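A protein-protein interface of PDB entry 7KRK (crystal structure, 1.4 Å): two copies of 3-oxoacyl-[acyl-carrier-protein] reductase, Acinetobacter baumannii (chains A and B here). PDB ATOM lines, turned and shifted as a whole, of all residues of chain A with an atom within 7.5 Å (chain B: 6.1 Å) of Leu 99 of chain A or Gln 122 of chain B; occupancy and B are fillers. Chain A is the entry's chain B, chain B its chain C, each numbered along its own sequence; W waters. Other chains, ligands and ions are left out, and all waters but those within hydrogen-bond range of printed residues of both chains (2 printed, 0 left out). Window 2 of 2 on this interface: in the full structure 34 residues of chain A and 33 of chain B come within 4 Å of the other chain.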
ATOM      1  N   ILE A  96      -6.413  28.047 -10.871  1.00  0.00           N
ATOM      2  CA  ILE A  96      -7.531  28.653 -10.163  1.00  0.00           C
ATOM      3  C   ILE A  96      -7.944  27.740  -9.018  1.00  0.00           C
ATOM      4  O   ILE A  96      -7.823  26.514  -9.097  1.00  0.00           O
ATOM      5  CB  ILE A  96      -8.728  28.959 -11.088  1.00  0.00           C
ATOM      6  CG1 ILE A  96      -9.224  27.683 -11.764  1.00  0.00           C
ATOM      7  CG2 ILE A  96      -8.338  30.004 -12.128  1.00  0.00           C
ATOM      8  CD1 ILE A  96     -10.499  27.871 -12.557  1.00  0.00           C
ATOM      9  N   LYS A  97      -8.445  28.351  -7.953  1.00  0.00           N
ATOM     10  CA  LYS A  97      -8.743  27.642  -6.720  1.00  0.00           C
ATOM     11  C   LYS A  97     -10.178  27.114  -6.719  1.00  0.00           C
ATOM     12  O   LYS A  97     -10.989  27.425  -7.596  1.00  0.00           O
ATOM     13  CB  LYS A  97      -8.488  28.557  -5.523  1.00  0.00           C
ATOM     14  CG  LYS A  97      -7.046  29.033  -5.440  1.00  0.00           C
ATOM     15  CD  LYS A  97      -6.799  29.912  -4.227  1.00  0.00           C
ATOM     16  CE  LYS A  97      -5.335  30.316  -4.142  1.00  0.00           C
ATOM     17  NZ  LYS A  97      -5.054  31.193  -2.972  1.00  0.00           N
ATOM     18  N   THR A  98     -10.487  26.312  -5.696  1.00  0.00           N
ATOM     19  CA  THR A  98     -11.726  25.537  -5.676  1.00  0.00           C
ATOM     20  C   THR A  98     -12.946  26.397  -5.987  1.00  0.00           C
ATOM     21  O   THR A  98     -13.734  26.077  -6.883  1.00  0.00           O
ATOM     22  CB  THR A  98     -11.901  24.866  -4.309  1.00  0.00           C
ATOM     23  OG1 THR A  98     -10.822  23.958  -4.062  1.00  0.00           O
ATOM     24  CG2 THR A  98     -13.213  24.096  -4.259  1.00  0.00           C
ATOM     25  N   LEU A  99     -13.133  27.483  -5.238  1.00  0.00           N
ATOM     26  CA  LEU A  99     -14.378  28.235  -5.331  1.00  0.00           C
ATOM     27  C   LEU A  99     -14.496  29.037  -6.619  1.00  0.00           C
ATOM     28  O   LEU A  99     -15.585  29.541  -6.913  1.00  0.00           O
ATOM     29  CB  LEU A  99     -14.522  29.163  -4.123  1.00  0.00           C
ATOM     30  CG  LEU A  99     -14.573  28.458  -2.765  1.00  0.00           C
ATOM     31  CD1 LEU A  99     -14.704  29.473  -1.639  1.00  0.00           C
ATOM     32  CD2 LEU A  99     -15.714  27.449  -2.709  1.00  0.00           C
ATOM     33  N   ASP A 100     -13.423  29.154  -7.394  1.00  0.00           N
ATOM     34  CA  ASP A 100     -13.437  29.934  -8.622  1.00  0.00           C
ATOM     35  C   ASP A 100     -13.619  29.083  -9.872  1.00  0.00           C
ATOM     36  O   ASP A 100     -13.675  29.633 -10.975  1.00  0.00           O
ATOM     37  CB  ASP A 100     -12.154  30.762  -8.727  1.00  0.00           C
ATOM     38  CG  ASP A 100     -12.037  31.790  -7.614  1.00  0.00           C
ATOM     39  OD1 ASP A 100     -13.068  32.398  -7.259  1.00  0.00           O
ATOM     40  OD2 ASP A 100     -10.920  31.981  -7.091  1.00  0.00           O
ATOM     41  N   ILE A 101     -13.730  27.764  -9.733  1.00  0.00           N
ATOM     42  CA  ILE A 101     -13.872  26.880 -10.888  1.00  0.00           C
ATOM     43  C   ILE A 101     -15.301  26.986 -11.411  1.00  0.00           C
ATOM     44  O   ILE A 101     -16.251  26.590 -10.731  1.00  0.00           O
ATOM     45  CB  ILE A 101     -13.525  25.432 -10.532  1.00  0.00           C
ATOM     46  CG1 ILE A 101     -12.070  25.321 -10.081  1.00  0.00           C
ATOM     47  CG2 ILE A 101     -13.777  24.524 -11.732  1.00  0.00           C
ATOM     48  CD1 ILE A 101     -11.762  24.032  -9.345  1.00  0.00           C
ATOM     49  N   GLN A 102     -15.450  27.500 -12.628  1.00  0.00           N
ATOM     50  CA  GLN A 102     -16.743  27.602 -13.283  1.00  0.00           C
ATOM     51  C   GLN A 102     -16.967  26.395 -14.189  1.00  0.00           C
ATOM     52  O   GLN A 102     -16.044  25.645 -14.513  1.00  0.00           O
ATOM     53  CB  GLN A 102     -16.817  28.886 -14.109  1.00  0.00           C
ATOM     54  CG  GLN A 102     -16.416  30.139 -13.348  1.00  0.00           C
ATOM     55  CD  GLN A 102     -17.261  30.371 -12.112  1.00  0.00           C
ATOM     56  OE1 GLN A 102     -16.735  30.623 -11.027  1.00  0.00           O
ATOM     57  NE2 GLN A 102     -18.577  30.294 -12.270  1.00  0.00           N
ATOM     58  N   ARG A 103     -18.222  26.220 -14.606  1.00  0.00           N
ATOM     59  CA  ARG A 103     -18.578  25.096 -15.466  1.00  0.00           C
ATOM     60  C   ARG A 103     -17.654  24.998 -16.673  1.00  0.00           C
ATOM     61  O   ARG A 103     -17.189  23.904 -17.021  1.00  0.00           O
ATOM     62  CB  ARG A 103     -20.033  25.237 -15.915  1.00  0.00           C
ATOM     63  CG  ARG A 103     -20.475  24.217 -16.951  1.00  0.00           C
ATOM     64  CD  ARG A 103     -21.988  24.211 -17.103  1.00  0.00           C
ATOM     65  NE  ARG A 103     -22.652  23.629 -15.938  1.00  0.00           N
ATOM     66  CZ  ARG A 103     -23.090  22.375 -15.855  1.00  0.00           C
ATOM     67  NH1 ARG A 103     -22.945  21.536 -16.874  1.00  0.00           N
ATOM     68  NH2 ARG A 103     -23.680  21.954 -14.746  1.00  0.00           N
ATOM     69  N   PRO A 154      -7.773  22.540  -8.429  1.00  0.00           N
ATOM     70  CA  PRO A 154      -8.386  21.259  -8.038  1.00  0.00           C
ATOM     71  C   PRO A 154      -9.045  20.503  -9.177  1.00  0.00           C
ATOM     72  O   PRO A 154      -9.093  19.269  -9.134  1.00  0.00           O
ATOM     73  CB  PRO A 154      -9.392  21.672  -6.954  1.00  0.00           C
ATOM     74  CG  PRO A 154      -8.801  22.915  -6.369  1.00  0.00           C
ATOM     75  CD  PRO A 154      -8.163  23.634  -7.523  1.00  0.00           C
ATOM     76  N   GLU B  66     -25.790  23.840 -10.636  1.00  0.00           N
ATOM     77  CA  GLU B  66     -25.183  24.778  -9.698  1.00  0.00           C
ATOM     78  C   GLU B  66     -26.233  25.590  -8.947  1.00  0.00           C
ATOM     79  O   GLU B  66     -26.194  25.690  -7.716  1.00  0.00           O
ATOM     80  CB  GLU B  66     -24.233  25.714 -10.448  1.00  0.00           C
ATOM     81  CG  GLU B  66     -22.993  25.038 -11.011  1.00  0.00           C
ATOM     82  CD  GLU B  66     -23.173  24.551 -12.435  1.00  0.00           C
ATOM     83  OE1 GLU B  66     -22.194  24.623 -13.209  1.00  0.00           O
ATOM     84  OE2 GLU B  66     -24.285  24.101 -12.784  1.00  0.00           O
ATOM     85  N   LYS B  70     -27.088  25.537  -4.945  1.00  0.00           N
ATOM     86  CA  LYS B  70     -26.900  26.725  -4.122  1.00  0.00           C
ATOM     87  C   LYS B  70     -28.190  27.110  -3.412  1.00  0.00           C
ATOM     88  O   LYS B  70     -28.173  27.480  -2.232  1.00  0.00           O
ATOM     89  CB  LYS B  70     -26.384  27.877  -4.982  1.00  0.00           C
ATOM     90  CG  LYS B  70     -24.948  27.682  -5.451  1.00  0.00           C
ATOM     91  CD  LYS B  70     -24.521  28.758  -6.438  1.00  0.00           C
ATOM     92  CE  LYS B  70     -23.094  28.533  -6.919  1.00  0.00           C
ATOM     93  NZ  LYS B  70     -22.618  29.630  -7.805  1.00  0.00           N
ATOM     94  N   THR B 117     -19.826  16.507  -6.708  1.00  0.00           N
ATOM     95  CA  THR B 117     -18.978  16.709  -5.538  1.00  0.00           C
ATOM     96  C   THR B 117     -18.355  18.099  -5.550  1.00  0.00           C
ATOM     97  O   THR B 117     -18.300  18.771  -4.513  1.00  0.00           O
ATOM     98  CB  THR B 117     -17.904  15.622  -5.467  1.00  0.00           C
ATOM     99  OG1 THR B 117     -18.517  14.367  -5.152  1.00  0.00           O
ATOM    100  CG2 THR B 117     -16.870  15.947  -4.397  1.00  0.00           C
ATOM    101  N   LEU B 118     -17.892  18.557  -6.715  1.00  0.00           N
ATOM    102  CA  LEU B 118     -17.341  19.904  -6.804  1.00  0.00           C
ATOM    103  C   LEU B 118     -18.402  20.947  -6.473  1.00  0.00           C
ATOM    104  O   LEU B 118     -18.176  21.842  -5.651  1.00  0.00           O
ATOM    105  CB  LEU B 118     -16.777  20.148  -8.203  1.00  0.00           C
ATOM    106  CG  LEU B 118     -16.264  21.568  -8.467  1.00  0.00           C
ATOM    107  CD1 LEU B 118     -15.115  21.916  -7.534  1.00  0.00           C
ATOM    108  CD2 LEU B 118     -15.840  21.711  -9.917  1.00  0.00           C
ATOM    109  N   ILE B 119     -19.573  20.837  -7.101  1.00  0.00           N
ATOM    110  CA  ILE B 119     -20.605  21.860  -6.952  1.00  0.00           C
ATOM    111  C   ILE B 119     -21.102  21.922  -5.513  1.00  0.00           C
ATOM    112  O   ILE B 119     -21.223  23.004  -4.927  1.00  0.00           O
ATOM    113  CB  ILE B 119     -21.749  21.610  -7.950  1.00  0.00           C
ATOM    114  CG1 ILE B 119     -21.286  21.955  -9.367  1.00  0.00           C
ATOM    115  CG2 ILE B 119     -22.984  22.416  -7.557  1.00  0.00           C
ATOM    116  CD1 ILE B 119     -22.228  21.487 -10.459  1.00  0.00           C
ATOM    117  N   MET B 120     -21.406  20.765  -4.921  1.00  0.00           N
ATOM    118  CA  MET B 120     -21.907  20.766  -3.551  1.00  0.00           C
ATOM    119  C   MET B 120     -20.836  21.238  -2.578  1.00  0.00           C
ATOM    120  O   MET B 120     -21.133  21.975  -1.631  1.00  0.00           O
ATOM    121  CB  MET B 120     -22.426  19.382  -3.162  1.00  0.00           C
ATOM    122  CG  MET B 120     -23.012  19.324  -1.752  1.00  0.00           C
ATOM    123  SD  MET B 120     -24.382  20.470  -1.457  1.00  0.00           S
ATOM    124  CE  MET B 120     -25.678  19.655  -2.382  1.00  0.00           C
ATOM    125  N   SER B 121     -19.583  20.830  -2.792  1.00  0.00           N
ATOM    126  CA  SER B 121     -18.507  21.319  -1.937  1.00  0.00           C
ATOM    127  C   SER B 121     -18.344  22.828  -2.079  1.00  0.00           C
ATOM    128  O   SER B 121     -18.195  23.541  -1.078  1.00  0.00           O
ATOM    129  CB  SER B 121     -17.201  20.599  -2.271  1.00  0.00           C
ATOM    130  OG  SER B 121     -17.296  19.214  -1.984  1.00  0.00           O
ATOM    131  N   GLN B 122     -18.376  23.336  -3.314  1.00  0.00           N
ATOM    132  CA  GLN B 122     -18.308  24.779  -3.526  1.00  0.00           C
ATOM    133  C   GLN B 122     -19.427  25.499  -2.788  1.00  0.00           C
ATOM    134  O   GLN B 122     -19.233  26.609  -2.278  1.00  0.00           O
ATOM    135  CB  GLN B 122     -18.405  25.098  -5.017  1.00  0.00           C
ATOM    136  CG  GLN B 122     -17.156  24.809  -5.817  1.00  0.00           C
ATOM    137  CD  GLN B 122     -17.354  25.072  -7.295  1.00  0.00           C
ATOM    138  OE1 GLN B 122     -18.414  24.781  -7.852  1.00  0.00           O
ATOM    139  NE2 GLN B 122     -16.339  25.634  -7.938  1.00  0.00           N
ATOM    140  N   ALA B 123     -20.611  24.888  -2.730  1.00  0.00           N
ATOM    141  CA  ALA B 123     -21.761  25.556  -2.132  1.00  0.00           C
ATOM    142  C   ALA B 123     -21.672  25.599  -0.611  1.00  0.00           C
ATOM    143  O   ALA B 123     -22.211  26.520   0.009  1.00  0.00           O
ATOM    144  CB  ALA B 123     -23.052  24.863  -2.562  1.00  0.00           C
ATOM    145  N   VAL B 124     -20.993  24.631   0.003  1.00  0.00           N
ATOM    146  CA  VAL B 124     -20.980  24.492   1.456  1.00  0.00           C
ATOM    147  C   VAL B 124     -19.721  25.101   2.065  1.00  0.00           C
ATOM    148  O   VAL B 124     -19.741  25.573   3.208  1.00  0.00           O
ATOM    149  CB  VAL B 124     -21.126  23.010   1.852  1.00  0.00           C
ATOM    150  CG1 VAL B 124     -20.974  22.837   3.348  1.00  0.00           C
ATOM    151  CG2 VAL B 124     -22.467  22.471   1.389  1.00  0.00           C
ATOM    152  N   ILE B 125     -18.622  25.102   1.307  1.00  0.00           N
ATOM    153  CA  ILE B 125     -17.341  25.558   1.860  1.00  0.00           C
ATOM    154  C   ILE B 125     -17.402  26.977   2.406  1.00  0.00           C
ATOM    155  O   ILE B 125     -16.839  27.225   3.483  1.00  0.00           O
ATOM    156  CB  ILE B 125     -16.211  25.322   0.850  1.00  0.00           C
ATOM    157  CG1 ILE B 125     -15.795  23.849   0.873  1.00  0.00           C
ATOM    158  CG2 ILE B 125     -15.017  26.226   1.147  1.00  0.00           C
ATOM    159  CD1 ILE B 125     -14.925  23.433  -0.295  1.00  0.00           C
ATOM    160  N   PRO B 126     -18.030  27.949   1.741  1.00  0.00           N
ATOM    161  CA  PRO B 126     -18.044  29.311   2.303  1.00  0.00           C
ATOM    162  C   PRO B 126     -18.576  29.377   3.725  1.00  0.00           C
ATOM    163  O   PRO B 126     -17.971  30.040   4.580  1.00  0.00           O
ATOM    164  CB  PRO B 126     -18.902  30.089   1.298  1.00  0.00           C
ATOM    165  CG  PRO B 126     -18.703  29.362   0.010  1.00  0.00           C
ATOM    166  CD  PRO B 126     -18.609  27.910   0.386  1.00  0.00           C
ATOM    167  N   LYS B 129     -16.013  27.860   6.155  1.00  0.00           N
ATOM    168  CA  LYS B 129     -14.969  28.827   6.474  1.00  0.00           C
ATOM    169  C   LYS B 129     -15.457  29.822   7.519  1.00  0.00           C
ATOM    170  O   LYS B 129     -14.765  30.101   8.503  1.00  0.00           O
ATOM    171  CB  LYS B 129     -14.528  29.565   5.211  1.00  0.00           C
ATOM    172  CG  LYS B 129     -13.716  28.729   4.241  1.00  0.00           C
ATOM    173  CD  LYS B 129     -13.188  29.564   3.076  1.00  0.00           C
ATOM    174  CE  LYS B 129     -12.237  30.659   3.543  1.00  0.00           C
ATOM    175  NZ  LYS B 129     -11.534  31.318   2.408  1.00  0.00           N
ATOM    176  N   MET B 170      -8.797  19.764  -2.346  1.00  0.00           N
ATOM    177  CA  MET B 170      -9.549  20.605  -1.420  1.00  0.00           C
ATOM    178  C   MET B 170      -9.019  20.465   0.000  1.00  0.00           C
ATOM    179  O   MET B 170      -8.961  21.449   0.746  1.00  0.00           O
ATOM    180  CB  MET B 170     -11.036  20.261  -1.484  1.00  0.00           C
ATOM    181  CG  MET B 170     -11.675  20.564  -2.832  1.00  0.00           C
ATOM    182  SD  MET B 170     -13.482  20.508  -2.825  1.00  0.00           S
ATOM    183  CE  MET B 170     -13.782  18.815  -2.327  1.00  0.00           C
ATOM    184  N   GLU B 173      -6.067  22.746   0.125  1.00  0.00           N
ATOM    185  CA  GLU B 173      -6.401  24.164   0.044  1.00  0.00           C
ATOM    186  C   GLU B 173      -6.999  24.680   1.348  1.00  0.00           C
ATOM    187  O   GLU B 173      -6.686  25.797   1.776  1.00  0.00           O
ATOM    188  CB  GLU B 173      -7.356  24.445  -1.120  1.00  0.00           C
ATOM    189  CG  GLU B 173      -7.801  25.911  -1.156  1.00  0.00           C
ATOM    190  CD  GLU B 173      -8.581  26.303  -2.397  1.00  0.00           C
ATOM    191  OE1 GLU B 173      -8.715  25.481  -3.328  1.00  0.00           O
ATOM    192  OE2 GLU B 173      -9.062  27.455  -2.437  1.00  0.00           O
ATOM    193  N   PHE B 174      -7.857  23.891   1.993  1.00  0.00           N
ATOM    194  CA  PHE B 174      -8.672  24.382   3.098  1.00  0.00           C
ATOM    195  C   PHE B 174      -8.227  23.873   4.464  1.00  0.00           C
ATOM    196  O   PHE B 174      -8.938  24.086   5.454  1.00  0.00           O
ATOM    197  CB  PHE B 174     -10.147  24.073   2.836  1.00  0.00           C
ATOM    198  CG  PHE B 174     -10.693  24.774   1.626  1.00  0.00           C
ATOM    199  CD1 PHE B 174     -10.935  26.138   1.658  1.00  0.00           C
ATOM    200  CD2 PHE B 174     -10.928  24.086   0.448  1.00  0.00           C
ATOM    201  CE1 PHE B 174     -11.421  26.798   0.548  1.00  0.00           C
ATOM    202  CE2 PHE B 174     -11.414  24.742  -0.668  1.00  0.00           C
ATOM    203  CZ  PHE B 174     -11.659  26.101  -0.617  1.00  0.00           C
HETATM  204  O   HOH W   1     -11.288  28.639  -3.346  1.00  0.00           O
HETATM  205  O   HOH W   2     -18.392  24.433 -10.861  1.00  0.00           O
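O of Thr 98 of chain A lies within hydrogen-bond range of NE2 of Gln 122 of chain B (2.8 Å).
OE1 of Glu 173 of chain B lies within hydrogen-bond range of OG1 of Thr 98 of chain A, at 2.7 Å.
The backbone carbonyl oxygen of Ile 101 of chain A lies within hydrogen-bond range of the side-chain amide nitrogen of Gln 122 of chain B.
OE1 of Glu 66 of chain B lies within salt-bridge range of NE of Arg 103 of chain A, 2.9 Å away.
Water W1 lies within hydrogen-bond range of OE2 of Glu 173 of chain B, N of Leu 99 of chain A and N of Thr 98 of chain A.
Water W2 bridges OE1 of Gln 122 of chain B and O of Ile 101 of chain A.
Of the printed residues of chain B, Lys 97 of chain A touches Glu 173.
Leu 99 of chain A touches one residue of chain B.
Of the printed residues of chain B, Arg 103 of chain A touches Glu 66.
Of the printed residues of chain A, Leu 118 of chain B touches Ile 101 (3.9 Å).
Of the printed residues of chain A, Gln 122 of chain B touches Thr 98, Leu 99 and Ile 101.
Printed residues of chain A within 4 Å of Glu 173 of chain B: Lys 97, Thr 98 and Pro 154.
The nearest residue of chain B that does not touch Leu 99 of chain A is Ile 125 of chain B (4.1 Å).
The nearest printed residue of chain B that does not touch Ile 101 of chain A is Glu 66 of chain B (6.7 Å).
Hydrophobic or aromatic side chains of chain B within 4 Å of the printed part of chain A: Leu 118, Met 170 and Phe 174.
Hydrophobic or aromatic side chains of chain A that line the printed part of chain B: Leu 99, Ile 101 and Pro 154.
Among the printed residues, pairs that only touch across the chains: Lys 97 of chain A with Glu 173 of chain B (3.3 Å), Thr 98 of chain A with Phe 174 of chain B (3.5 Å), Leu 99 of chain A with Gln 122 of chain B (3.6 Å), Thr 98 of chain A with Met 170 of chain B (3.7 Å), Ile 101 of chain A with Leu 118 of chain B (3.9 Å) and Pro 154 of chain A with Glu 173 of chain B (3.98 Å).
No position is printed for both chains.
Of the 10 pairs that touch across the chains among the printed residues, none has its exchanged pair printed and touching as well.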
